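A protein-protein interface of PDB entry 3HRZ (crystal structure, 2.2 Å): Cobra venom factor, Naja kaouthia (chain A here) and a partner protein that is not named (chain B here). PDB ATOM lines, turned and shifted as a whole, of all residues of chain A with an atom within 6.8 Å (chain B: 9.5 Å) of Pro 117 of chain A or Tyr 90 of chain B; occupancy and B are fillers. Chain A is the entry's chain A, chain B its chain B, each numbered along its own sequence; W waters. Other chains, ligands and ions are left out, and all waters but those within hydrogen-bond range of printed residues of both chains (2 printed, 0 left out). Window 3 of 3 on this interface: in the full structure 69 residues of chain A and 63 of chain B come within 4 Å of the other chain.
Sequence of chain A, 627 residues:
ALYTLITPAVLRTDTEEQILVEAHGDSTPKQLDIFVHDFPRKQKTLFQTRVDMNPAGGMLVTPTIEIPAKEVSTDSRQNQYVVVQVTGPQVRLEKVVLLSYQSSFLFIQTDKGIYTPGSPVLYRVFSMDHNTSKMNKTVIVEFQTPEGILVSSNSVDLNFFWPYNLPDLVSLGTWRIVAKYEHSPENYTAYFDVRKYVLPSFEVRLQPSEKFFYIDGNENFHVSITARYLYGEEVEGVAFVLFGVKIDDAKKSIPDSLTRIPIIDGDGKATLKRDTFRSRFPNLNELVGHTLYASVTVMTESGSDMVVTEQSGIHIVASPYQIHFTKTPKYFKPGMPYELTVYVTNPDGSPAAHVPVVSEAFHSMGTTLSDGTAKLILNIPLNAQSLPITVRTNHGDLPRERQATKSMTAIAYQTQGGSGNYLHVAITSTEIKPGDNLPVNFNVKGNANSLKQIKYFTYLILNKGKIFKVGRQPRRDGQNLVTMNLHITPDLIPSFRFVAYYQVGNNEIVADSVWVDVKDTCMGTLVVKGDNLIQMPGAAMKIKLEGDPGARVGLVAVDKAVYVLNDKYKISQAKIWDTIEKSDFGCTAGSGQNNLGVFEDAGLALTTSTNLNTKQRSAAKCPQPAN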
ATOM      1  N   TYR A 115       9.123  18.543 -28.613  1.00  0.00           N
ATOM      2  CA  TYR A 115       9.194  19.226 -27.323  1.00  0.00           C
ATOM      3  C   TYR A 115      10.379  18.742 -26.492  1.00  0.00           C
ATOM      4  O   TYR A 115      10.812  17.588 -26.623  1.00  0.00           O
ATOM      5  CB  TYR A 115       7.902  18.995 -26.527  1.00  0.00           C
ATOM      6  CG  TYR A 115       6.658  19.529 -27.201  1.00  0.00           C
ATOM      7  CD1 TYR A 115       6.096  20.737 -26.805  1.00  0.00           C
ATOM      8  CD2 TYR A 115       6.049  18.823 -28.250  1.00  0.00           C
ATOM      9  CE1 TYR A 115       4.965  21.237 -27.424  1.00  0.00           C
ATOM     10  CE2 TYR A 115       4.921  19.320 -28.881  1.00  0.00           C
ATOM     11  CZ  TYR A 115       4.376  20.526 -28.466  1.00  0.00           C
ATOM     12  OH  TYR A 115       3.238  21.018 -29.082  1.00  0.00           O
ATOM     13  N   THR A 116      10.879  19.617 -25.619  1.00  0.00           N
ATOM     14  CA  THR A 116      11.877  19.223 -24.633  1.00  0.00           C
ATOM     15  C   THR A 116      11.192  18.820 -23.331  1.00  0.00           C
ATOM     16  O   THR A 116      10.082  19.259 -23.051  1.00  0.00           O
ATOM     17  CB  THR A 116      12.859  20.375 -24.316  1.00  0.00           C
ATOM     18  OG1 THR A 116      12.128  21.531 -23.887  1.00  0.00           O
ATOM     19  CG2 THR A 116      13.685  20.739 -25.539  1.00  0.00           C
ATOM     20  N   PRO A 117      11.855  17.979 -22.526  1.00  0.00           N
ATOM     21  CA  PRO A 117      11.353  17.651 -21.187  1.00  0.00           C
ATOM     22  C   PRO A 117      10.964  18.895 -20.386  1.00  0.00           C
ATOM     23  O   PRO A 117      11.538  19.966 -20.573  1.00  0.00           O
ATOM     24  CB  PRO A 117      12.563  16.979 -20.527  1.00  0.00           C
ATOM     25  CG  PRO A 117      13.238  16.292 -21.661  1.00  0.00           C
ATOM     26  CD  PRO A 117      13.090  17.242 -22.844  1.00  0.00           C
ATOM     27  N   GLY A 118       9.991  18.740 -19.500  1.00  0.00           N
ATOM     28  CA  GLY A 118       9.577  19.827 -18.627  1.00  0.00           C
ATOM     29  C   GLY A 118       8.830  20.980 -19.285  1.00  0.00           C
ATOM     30  O   GLY A 118       8.802  22.084 -18.742  1.00  0.00           O
ATOM     31  N   SER A 119       8.219  20.740 -20.441  1.00  0.00           N
ATOM     32  CA  SER A 119       7.532  21.817 -21.144  1.00  0.00           C
ATOM     33  C   SER A 119       6.082  21.456 -21.485  1.00  0.00           C
ATOM     34  O   SER A 119       5.743  20.281 -21.575  1.00  0.00           O
ATOM     35  CB  SER A 119       8.306  22.219 -22.406  1.00  0.00           C
ATOM     36  OG  SER A 119       8.326  21.153 -23.338  1.00  0.00           O
ATOM     37  N   LEU A 166       4.651  18.313 -19.730  1.00  0.00           N
ATOM     38  CA  LEU A 166       5.607  17.214 -19.772  1.00  0.00           C
ATOM     39  C   LEU A 166       6.510  17.279 -18.539  1.00  0.00           C
ATOM     40  O   LEU A 166       7.045  18.341 -18.211  1.00  0.00           O
ATOM     41  CB  LEU A 166       6.456  17.307 -21.038  1.00  0.00           C
ATOM     42  CG  LEU A 166       5.808  17.054 -22.404  1.00  0.00           C
ATOM     43  CD1 LEU A 166       6.767  17.437 -23.517  1.00  0.00           C
ATOM     44  CD2 LEU A 166       5.377  15.598 -22.553  1.00  0.00           C
ATOM     45  N   PRO A 167       6.680  16.146 -17.843  1.00  0.00           N
ATOM     46  CA  PRO A 167       7.580  16.116 -16.676  1.00  0.00           C
ATOM     47  C   PRO A 167       9.040  16.313 -17.099  1.00  0.00           C
ATOM     48  O   PRO A 167       9.365  16.183 -18.286  1.00  0.00           O
ATOM     49  CB  PRO A 167       7.401  14.703 -16.112  1.00  0.00           C
ATOM     50  CG  PRO A 167       6.268  14.072 -16.902  1.00  0.00           C
ATOM     51  CD  PRO A 167       6.113  14.828 -18.171  1.00  0.00           C
ATOM     52  N   ASP A 168       9.909  16.620 -16.143  1.00  0.00           N
ATOM     53  CA  ASP A 168      11.330  16.789 -16.451  1.00  0.00           C
ATOM     54  C   ASP A 168      12.026  15.447 -16.568  1.00  0.00           C
ATOM     55  O   ASP A 168      12.980  15.292 -17.322  1.00  0.00           O
ATOM     56  CB  ASP A 168      12.010  17.683 -15.421  1.00  0.00           C
ATOM     57  CG  ASP A 168      11.950  19.148 -15.808  1.00  0.00           C
ATOM     58  OD1 ASP A 168      12.503  19.507 -16.877  1.00  0.00           O
ATOM     59  OD2 ASP A 168      11.344  19.939 -15.058  1.00  0.00           O
ATOM     60  N   LEU A 169      11.536  14.474 -15.814  1.00  0.00           N
ATOM     61  CA  LEU A 169      11.941  13.088 -15.993  1.00  0.00           C
ATOM     62  C   LEU A 169      10.839  12.458 -16.820  1.00  0.00           C
ATOM     63  O   LEU A 169       9.772  12.128 -16.316  1.00  0.00           O
ATOM     64  CB  LEU A 169      12.090  12.380 -14.647  1.00  0.00           C
ATOM     65  CG  LEU A 169      13.270  12.878 -13.809  1.00  0.00           C
ATOM     66  CD1 LEU A 169      13.163  12.414 -12.368  1.00  0.00           C
ATOM     67  CD2 LEU A 169      14.594  12.437 -14.426  1.00  0.00           C
ATOM     68  N   VAL A 170      11.087  12.326 -18.112  1.00  0.00           N
ATOM     69  CA  VAL A 170      10.009  12.004 -19.034  1.00  0.00           C
ATOM     70  C   VAL A 170      10.523  11.028 -20.066  1.00  0.00           C
ATOM     71  O   VAL A 170      11.698  11.066 -20.426  1.00  0.00           O
ATOM     72  CB  VAL A 170       9.471  13.285 -19.723  1.00  0.00           C
ATOM     73  CG1 VAL A 170      10.475  13.815 -20.757  1.00  0.00           C
ATOM     74  CG2 VAL A 170       8.136  13.018 -20.365  1.00  0.00           C
ATOM     75  N   LEU A 172      11.491   9.689 -23.449  1.00  0.00           N
ATOM     76  CA  LEU A 172      11.853  10.311 -24.724  1.00  0.00           C
ATOM     77  C   LEU A 172      11.323   9.487 -25.894  1.00  0.00           C
ATOM     78  O   LEU A 172      11.157   8.264 -25.786  1.00  0.00           O
ATOM     79  CB  LEU A 172      13.384  10.469 -24.848  1.00  0.00           C
ATOM     80  CG  LEU A 172      14.068  11.215 -23.699  1.00  0.00           C
ATOM     81  CD1 LEU A 172      15.575  11.298 -23.898  1.00  0.00           C
ATOM     82  CD2 LEU A 172      13.475  12.603 -23.557  1.00  0.00           C
ATOM     83  N   VAL A 194       9.399  13.971 -28.073  1.00  0.00           N
ATOM     84  CA  VAL A 194      10.008  14.578 -26.897  1.00  0.00           C
ATOM     85  C   VAL A 194      11.488  14.202 -26.933  1.00  0.00           C
ATOM     86  O   VAL A 194      11.833  13.025 -26.961  1.00  0.00           O
ATOM     87  CB  VAL A 194       9.307  14.132 -25.585  1.00  0.00           C
ATOM     88  CG1 VAL A 194      10.038  14.677 -24.345  1.00  0.00           C
ATOM     89  CG2 VAL A 194       7.854  14.597 -25.583  1.00  0.00           C
ATOM     90  N   ARG A 195      12.351  15.214 -26.998  1.00  0.00           N
ATOM     91  CA  ARG A 195      13.790  15.014 -27.181  1.00  0.00           C
ATOM     92  C   ARG A 195      14.538  16.083 -26.419  1.00  0.00           C
ATOM     93  O   ARG A 195      14.001  17.163 -26.182  1.00  0.00           O
ATOM     94  CB  ARG A 195      14.177  15.154 -28.664  1.00  0.00           C
ATOM     95  CG  ARG A 195      13.428  14.251 -29.632  1.00  0.00           C
ATOM     96  CD  ARG A 195      13.940  12.803 -29.627  1.00  0.00           C
ATOM     97  NE  ARG A 195      13.184  11.964 -30.560  1.00  0.00           N
ATOM     98  CZ  ARG A 195      13.238  10.633 -30.597  1.00  0.00           C
ATOM     99  NH1 ARG A 195      14.017   9.972 -29.748  1.00  0.00           N
ATOM    100  NH2 ARG A 195      12.505   9.961 -31.485  1.00  0.00           N
ATOM    101  N   LYS A 196      15.792  15.802 -26.087  1.00  0.00           N
ATOM    102  CA  LYS A 196      16.684  16.809 -25.532  1.00  0.00           C
ATOM    103  C   LYS A 196      17.406  17.515 -26.669  1.00  0.00           C
ATOM    104  O   LYS A 196      18.473  17.099 -27.101  1.00  0.00           O
ATOM    105  CB  LYS A 196      17.678  16.167 -24.565  1.00  0.00           C
ATOM    106  CG  LYS A 196      16.981  15.430 -23.425  1.00  0.00           C
ATOM    107  CD  LYS A 196      17.969  14.911 -22.392  1.00  0.00           C
ATOM    108  CE  LYS A 196      17.227  14.443 -21.139  1.00  0.00           C
ATOM    109  NZ  LYS A 196      18.145  13.977 -20.045  1.00  0.00           N
ATOM    110  N   TYR A 197      16.811  18.589 -27.158  1.00  0.00           N
ATOM    111  CA  TYR A 197      17.334  19.246 -28.334  1.00  0.00           C
ATOM    112  C   TYR A 197      17.450  20.725 -28.104  1.00  0.00           C
ATOM    113  O   TYR A 197      16.791  21.284 -27.216  1.00  0.00           O
ATOM    114  CB  TYR A 197      16.375  19.021 -29.505  1.00  0.00           C
ATOM    115  CG  TYR A 197      15.062  19.801 -29.426  1.00  0.00           C
ATOM    116  CD1 TYR A 197      14.951  21.083 -29.969  1.00  0.00           C
ATOM    117  CD2 TYR A 197      13.930  19.248 -28.831  1.00  0.00           C
ATOM    118  CE1 TYR A 197      13.750  21.797 -29.917  1.00  0.00           C
ATOM    119  CE2 TYR A 197      12.720  19.956 -28.771  1.00  0.00           C
ATOM    120  CZ  TYR A 197      12.636  21.228 -29.315  1.00  0.00           C
ATOM    121  OH  TYR A 197      11.442  21.928 -29.264  1.00  0.00           O
ATOM    122  N   VAL A 198      18.271  21.362 -28.926  1.00  0.00           N
ATOM    123  CA  VAL A 198      18.300  22.811 -28.997  1.00  0.00           C
ATOM    124  C   VAL A 198      18.048  23.180 -30.453  1.00  0.00           C
ATOM    125  O   VAL A 198      18.367  22.406 -31.353  1.00  0.00           O
ATOM    126  CB  VAL A 198      19.655  23.373 -28.541  1.00  0.00           C
ATOM    127  CG1 VAL A 198      20.054  22.778 -27.180  1.00  0.00           C
ATOM    128  CG2 VAL A 198      20.700  23.071 -29.564  1.00  0.00           C
ATOM    129  N   LYS B  21      10.271  28.977 -28.744  1.00  0.00           N
ATOM    130  CA  LYS B  21      10.162  28.095 -29.881  1.00  0.00           C
ATOM    131  C   LYS B  21       8.793  28.266 -30.518  1.00  0.00           C
ATOM    132  O   LYS B  21       8.635  28.117 -31.723  1.00  0.00           O
ATOM    133  CB  LYS B  21      10.363  26.656 -29.422  1.00  0.00           C
ATOM    134  CG  LYS B  21      11.766  26.396 -28.808  1.00  0.00           C
ATOM    135  CD  LYS B  21      11.890  24.926 -28.385  1.00  0.00           C
ATOM    136  CE  LYS B  21      13.205  24.597 -27.695  1.00  0.00           C
ATOM    137  NZ  LYS B  21      13.388  25.226 -26.346  1.00  0.00           N
ATOM    138  N   GLN B  87      24.979  29.464 -29.943  1.00  0.00           N
ATOM    139  CA  GLN B  87      24.490  28.095 -29.816  1.00  0.00           C
ATOM    140  C   GLN B  87      24.959  27.468 -28.507  1.00  0.00           C
ATOM    141  O   GLN B  87      26.158  27.377 -28.245  1.00  0.00           O
ATOM    142  CB  GLN B  87      24.946  27.236 -30.994  1.00  0.00           C
ATOM    143  CG  GLN B  87      24.237  27.567 -32.294  1.00  0.00           C
ATOM    144  CD  GLN B  87      22.723  27.438 -32.192  1.00  0.00           C
ATOM    145  OE1 GLN B  87      21.998  28.430 -32.321  1.00  0.00           O
ATOM    146  NE2 GLN B  87      22.239  26.212 -31.958  1.00  0.00           N
ATOM    147  N   MET B  88      24.008  27.048 -27.684  1.00  0.00           N
ATOM    148  CA  MET B  88      24.311  26.428 -26.403  1.00  0.00           C
ATOM    149  C   MET B  88      24.039  24.938 -26.514  1.00  0.00           C
ATOM    150  O   MET B  88      23.122  24.534 -27.213  1.00  0.00           O
ATOM    151  CB  MET B  88      23.411  27.009 -25.300  1.00  0.00           C
ATOM    152  CG  MET B  88      23.526  28.518 -25.074  1.00  0.00           C
ATOM    153  SD  MET B  88      24.892  29.008 -23.978  1.00  0.00           S
ATOM    154  CE  MET B  88      24.227  30.515 -23.281  1.00  0.00           C
ATOM    155  N   PRO B  89      24.823  24.121 -25.803  1.00  0.00           N
ATOM    156  CA  PRO B  89      24.577  22.682 -25.657  1.00  0.00           C
ATOM    157  C   PRO B  89      23.292  22.482 -24.854  1.00  0.00           C
ATOM    158  O   PRO B  89      22.875  23.393 -24.135  1.00  0.00           O
ATOM    159  CB  PRO B  89      25.777  22.223 -24.819  1.00  0.00           C
ATOM    160  CG  PRO B  89      26.113  23.447 -24.017  1.00  0.00           C
ATOM    161  CD  PRO B  89      25.977  24.558 -24.993  1.00  0.00           C
ATOM    162  N   TYR B  90      22.658  21.322 -24.966  1.00  0.00           N
ATOM    163  CA  TYR B  90      21.409  21.120 -24.244  1.00  0.00           C
ATOM    164  C   TYR B  90      21.654  21.230 -22.735  1.00  0.00           C
ATOM    165  O   TYR B  90      20.876  21.848 -22.019  1.00  0.00           O
ATOM    166  CB  TYR B  90      20.757  19.784 -24.601  1.00  0.00           C
ATOM    167  CG  TYR B  90      19.545  19.502 -23.753  1.00  0.00           C
ATOM    168  CD1 TYR B  90      18.291  20.008 -24.094  1.00  0.00           C
ATOM    169  CD2 TYR B  90      19.662  18.768 -22.572  1.00  0.00           C
ATOM    170  CE1 TYR B  90      17.171  19.761 -23.287  1.00  0.00           C
ATOM    171  CE2 TYR B  90      18.560  18.525 -21.760  1.00  0.00           C
ATOM    172  CZ  TYR B  90      17.322  19.022 -22.113  1.00  0.00           C
ATOM    173  OH  TYR B  90      16.243  18.754 -21.289  1.00  0.00           O
ATOM    174  N   SER B  91      22.740  20.624 -22.269  1.00  0.00           N
ATOM    175  CA  SER B  91      23.145  20.711 -20.866  1.00  0.00           C
ATOM    176  C   SER B  91      24.653  20.569 -20.725  1.00  0.00           C
ATOM    177  O   SER B  91      25.329  20.065 -21.628  1.00  0.00           O
ATOM    178  CB  SER B  91      22.475  19.610 -20.039  1.00  0.00           C
ATOM    179  OG  SER B  91      22.926  18.319 -20.429  1.00  0.00           O
ATOM    180  N   VAL B  92      25.162  21.003 -19.577  1.00  0.00           N
ATOM    181  CA  VAL B  92      26.570  20.843 -19.209  1.00  0.00           C
ATOM    182  C   VAL B  92      26.645  20.347 -17.765  1.00  0.00           C
ATOM    183  O   VAL B  92      25.662  20.448 -17.004  1.00  0.00           O
ATOM    184  CB  VAL B  92      27.376  22.157 -19.366  1.00  0.00           C
ATOM    185  CG1 VAL B  92      27.479  22.569 -20.863  1.00  0.00           C
ATOM    186  CG2 VAL B  92      26.769  23.281 -18.521  1.00  0.00           C
ATOM    187  N   VAL B  93      27.795  19.794 -17.386  1.00  0.00           N
ATOM    188  CA  VAL B  93      27.917  19.166 -16.086  1.00  0.00           C
ATOM    189  C   VAL B  93      28.578  20.110 -15.100  1.00  0.00           C
ATOM    190  O   VAL B  93      29.534  20.795 -15.437  1.00  0.00           O
ATOM    191  CB  VAL B  93      28.703  17.844 -16.171  1.00  0.00           C
ATOM    192  CG1 VAL B  93      28.956  17.282 -14.783  1.00  0.00           C
ATOM    193  CG2 VAL B  93      27.944  16.828 -17.044  1.00  0.00           C
ATOM    194  N   ILE B 100      32.145  27.659 -24.650  1.00  0.00           N
ATOM    195  CA  ILE B 100      30.954  28.114 -25.339  1.00  0.00           C
ATOM    196  C   ILE B 100      31.444  28.901 -26.548  1.00  0.00           C
ATOM    197  O   ILE B 100      32.283  29.791 -26.412  1.00  0.00           O
ATOM    198  CB  ILE B 100      30.114  29.052 -24.445  1.00  0.00           C
ATOM    199  CG1 ILE B 100      29.699  28.353 -23.150  1.00  0.00           C
ATOM    200  CG2 ILE B 100      28.881  29.498 -25.179  1.00  0.00           C
ATOM    201  CD1 ILE B 100      28.830  27.124 -23.374  1.00  0.00           C
ATOM    202  N   GLY B 158      21.483  23.757 -12.057  1.00  0.00           N
ATOM    203  CA  GLY B 158      20.323  24.546 -12.436  1.00  0.00           C
ATOM    204  C   GLY B 158      20.495  25.285 -13.758  1.00  0.00           C
ATOM    205  O   GLY B 158      21.317  24.905 -14.588  1.00  0.00           O
ATOM    206  N   LEU B 159      19.711  26.345 -13.947  1.00  0.00           N
ATOM    207  CA  LEU B 159      19.737  27.132 -15.174  1.00  0.00           C
ATOM    208  C   LEU B 159      20.309  28.490 -14.872  1.00  0.00           C
ATOM    209  O   LEU B 159      19.808  29.195 -14.005  1.00  0.00           O
ATOM    210  CB  LEU B 159      18.323  27.326 -15.716  1.00  0.00           C
ATOM    211  CG  LEU B 159      17.560  26.068 -16.113  1.00  0.00           C
ATOM    212  CD1 LEU B 159      16.114  26.414 -16.442  1.00  0.00           C
ATOM    213  CD2 LEU B 159      18.221  25.416 -17.300  1.00  0.00           C
ATOM    214  N   LYS B 180      20.023  30.964 -21.367  1.00  0.00           N
ATOM    215  CA  LYS B 180      20.103  30.083 -20.224  1.00  0.00           C
ATOM    216  C   LYS B 180      20.989  28.874 -20.501  1.00  0.00           C
ATOM    217  O   LYS B 180      20.866  28.219 -21.532  1.00  0.00           O
ATOM    218  CB  LYS B 180      18.699  29.642 -19.808  1.00  0.00           C
ATOM    219  CG  LYS B 180      17.896  30.741 -19.108  1.00  0.00           C
ATOM    220  CD  LYS B 180      16.422  30.357 -18.912  1.00  0.00           C
ATOM    221  CE  LYS B 180      15.626  30.473 -20.215  1.00  0.00           C
ATOM    222  NZ  LYS B 180      14.212  30.912 -19.981  1.00  0.00           N
ATOM    223  N   LEU B 181      21.892  28.595 -19.569  1.00  0.00           N
ATOM    224  CA  LEU B 181      22.704  27.395 -19.634  1.00  0.00           C
ATOM    225  C   LEU B 181      22.202  26.404 -18.597  1.00  0.00           C
ATOM    226  O   LEU B 181      22.050  26.748 -17.418  1.00  0.00           O
ATOM    227  CB  LEU B 181      24.170  27.730 -19.361  1.00  0.00           C
ATOM    228  CG  LEU B 181      25.106  26.531 -19.495  1.00  0.00           C
ATOM    229  CD1 LEU B 181      24.992  25.926 -20.894  1.00  0.00           C
ATOM    230  CD2 LEU B 181      26.541  26.913 -19.171  1.00  0.00           C
ATOM    231  N   LYS B 182      21.949  25.179 -19.038  1.00  0.00           N
ATOM    232  CA  LYS B 182      21.392  24.152 -18.181  1.00  0.00           C
ATOM    233  C   LYS B 182      22.514  23.332 -17.586  1.00  0.00           C
ATOM    234  O   LYS B 182      23.262  22.681 -18.315  1.00  0.00           O
ATOM    235  CB  LYS B 182      20.455  23.238 -18.970  1.00  0.00           C
ATOM    236  CG  LYS B 182      19.766  22.195 -18.082  1.00  0.00           C
ATOM    237  CD  LYS B 182      19.065  21.123 -18.901  1.00  0.00           C
ATOM    238  CE  LYS B 182      17.754  20.678 -18.249  1.00  0.00           C
ATOM    239  NZ  LYS B 182      17.912  20.071 -16.892  1.00  0.00           N
ATOM    240  N   VAL B 183      22.608  23.342 -16.263  1.00  0.00           N
ATOM    241  CA  VAL B 183      23.700  22.675 -15.562  1.00  0.00           C
ATOM    242  C   VAL B 183      23.174  21.501 -14.736  1.00  0.00           C
ATOM    243  O   VAL B 183      22.372  21.688 -13.833  1.00  0.00           O
ATOM    244  CB  VAL B 183      24.470  23.682 -14.642  1.00  0.00           C
ATOM    245  CG1 VAL B 183      25.609  23.000 -13.911  1.00  0.00           C
ATOM    246  CG2 VAL B 183      24.988  24.855 -15.459  1.00  0.00           C
ATOM    247  N   VAL B 184      23.632  20.293 -15.044  1.00  0.00           N
ATOM    248  CA  VAL B 184      23.208  19.116 -14.304  1.00  0.00           C
ATOM    249  C   VAL B 184      24.271  18.671 -13.299  1.00  0.00           C
ATOM    250  O   VAL B 184      25.449  18.963 -13.476  1.00  0.00           O
ATOM    251  CB  VAL B 184      22.899  17.962 -15.249  1.00  0.00           C
ATOM    252  CG1 VAL B 184      21.682  18.302 -16.114  1.00  0.00           C
ATOM    253  CG2 VAL B 184      24.117  17.649 -16.098  1.00  0.00           C
HETATM  254  O   HOH W   1      14.623  20.748 -21.219  1.00  0.00           O
HETATM  255  O   HOH W   2      16.273  23.729 -25.626  1.00  0.00           O
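Among the printed residues, pairs that only touch across the chains: Pro 117 of chain A with Tyr 90 of chain B, Lys 196 of chain A with Tyr 90 of chain B, Tyr 197 of chain A with Lys 21 of chain B, Tyr 197 of chain A with Tyr 90 of chain B, Val 198 of chain A with Met 88 of chain B, Val 198 of chain A with Pro 89 of chain B and Val 198 of chain A with Tyr 90 of chain B.
Water W1 lies within hydrogen-bond range of OH of Tyr 90 of chain B and O of Pro 117 of chain A.
Water W2 lies within hydrogen-bond range of O of Tyr 197 of chain A (3.0 Å) and NZ of Lys 21 of chain B (3.3 Å).
Pro 117 of chain A touches just one residue of chain B: Tyr 90.
Tyr 90 of chain B touches just these residues of chain A: Pro 117, Lys 196, Tyr 197 and Val 198.
No residue of chain B comes within 4 Å of Thr 116 of chain A.
Asp 168 of chain A touches none of the printed residues of chain B.
Of chain B, only Tyr 90 (3.7 Å) comes within 4 Å of Lys 196 of chain A.
Printed residues of chain A within 4 Å of Lys 21 of chain B: Tyr 197.
Of the printed residues of chain B, Tyr 197 of chain A touches Lys 21 and Tyr 90.
Val 93 of chain B touches none of the printed residues of chain A.
Of the 16 printed residues of chain A, 4 touch a printed residue of chain B.
Hydrophobic or aromatic side chains of chain A within 4 Å of the printed part of chain B: Pro 117, Tyr 197 and Val 198.
Along chain A the printed residues that touch a printed residue of chain B span positions 117 to 198.
Of the 16 printed residues of chain B, 4 touch a printed residue of chain A.
Hydrophobic or aromatic side chains of chain B within 4 Å of the printed part of chain A: Tyr 90.
Among the printed residues, 7 pairs touch across the chains.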
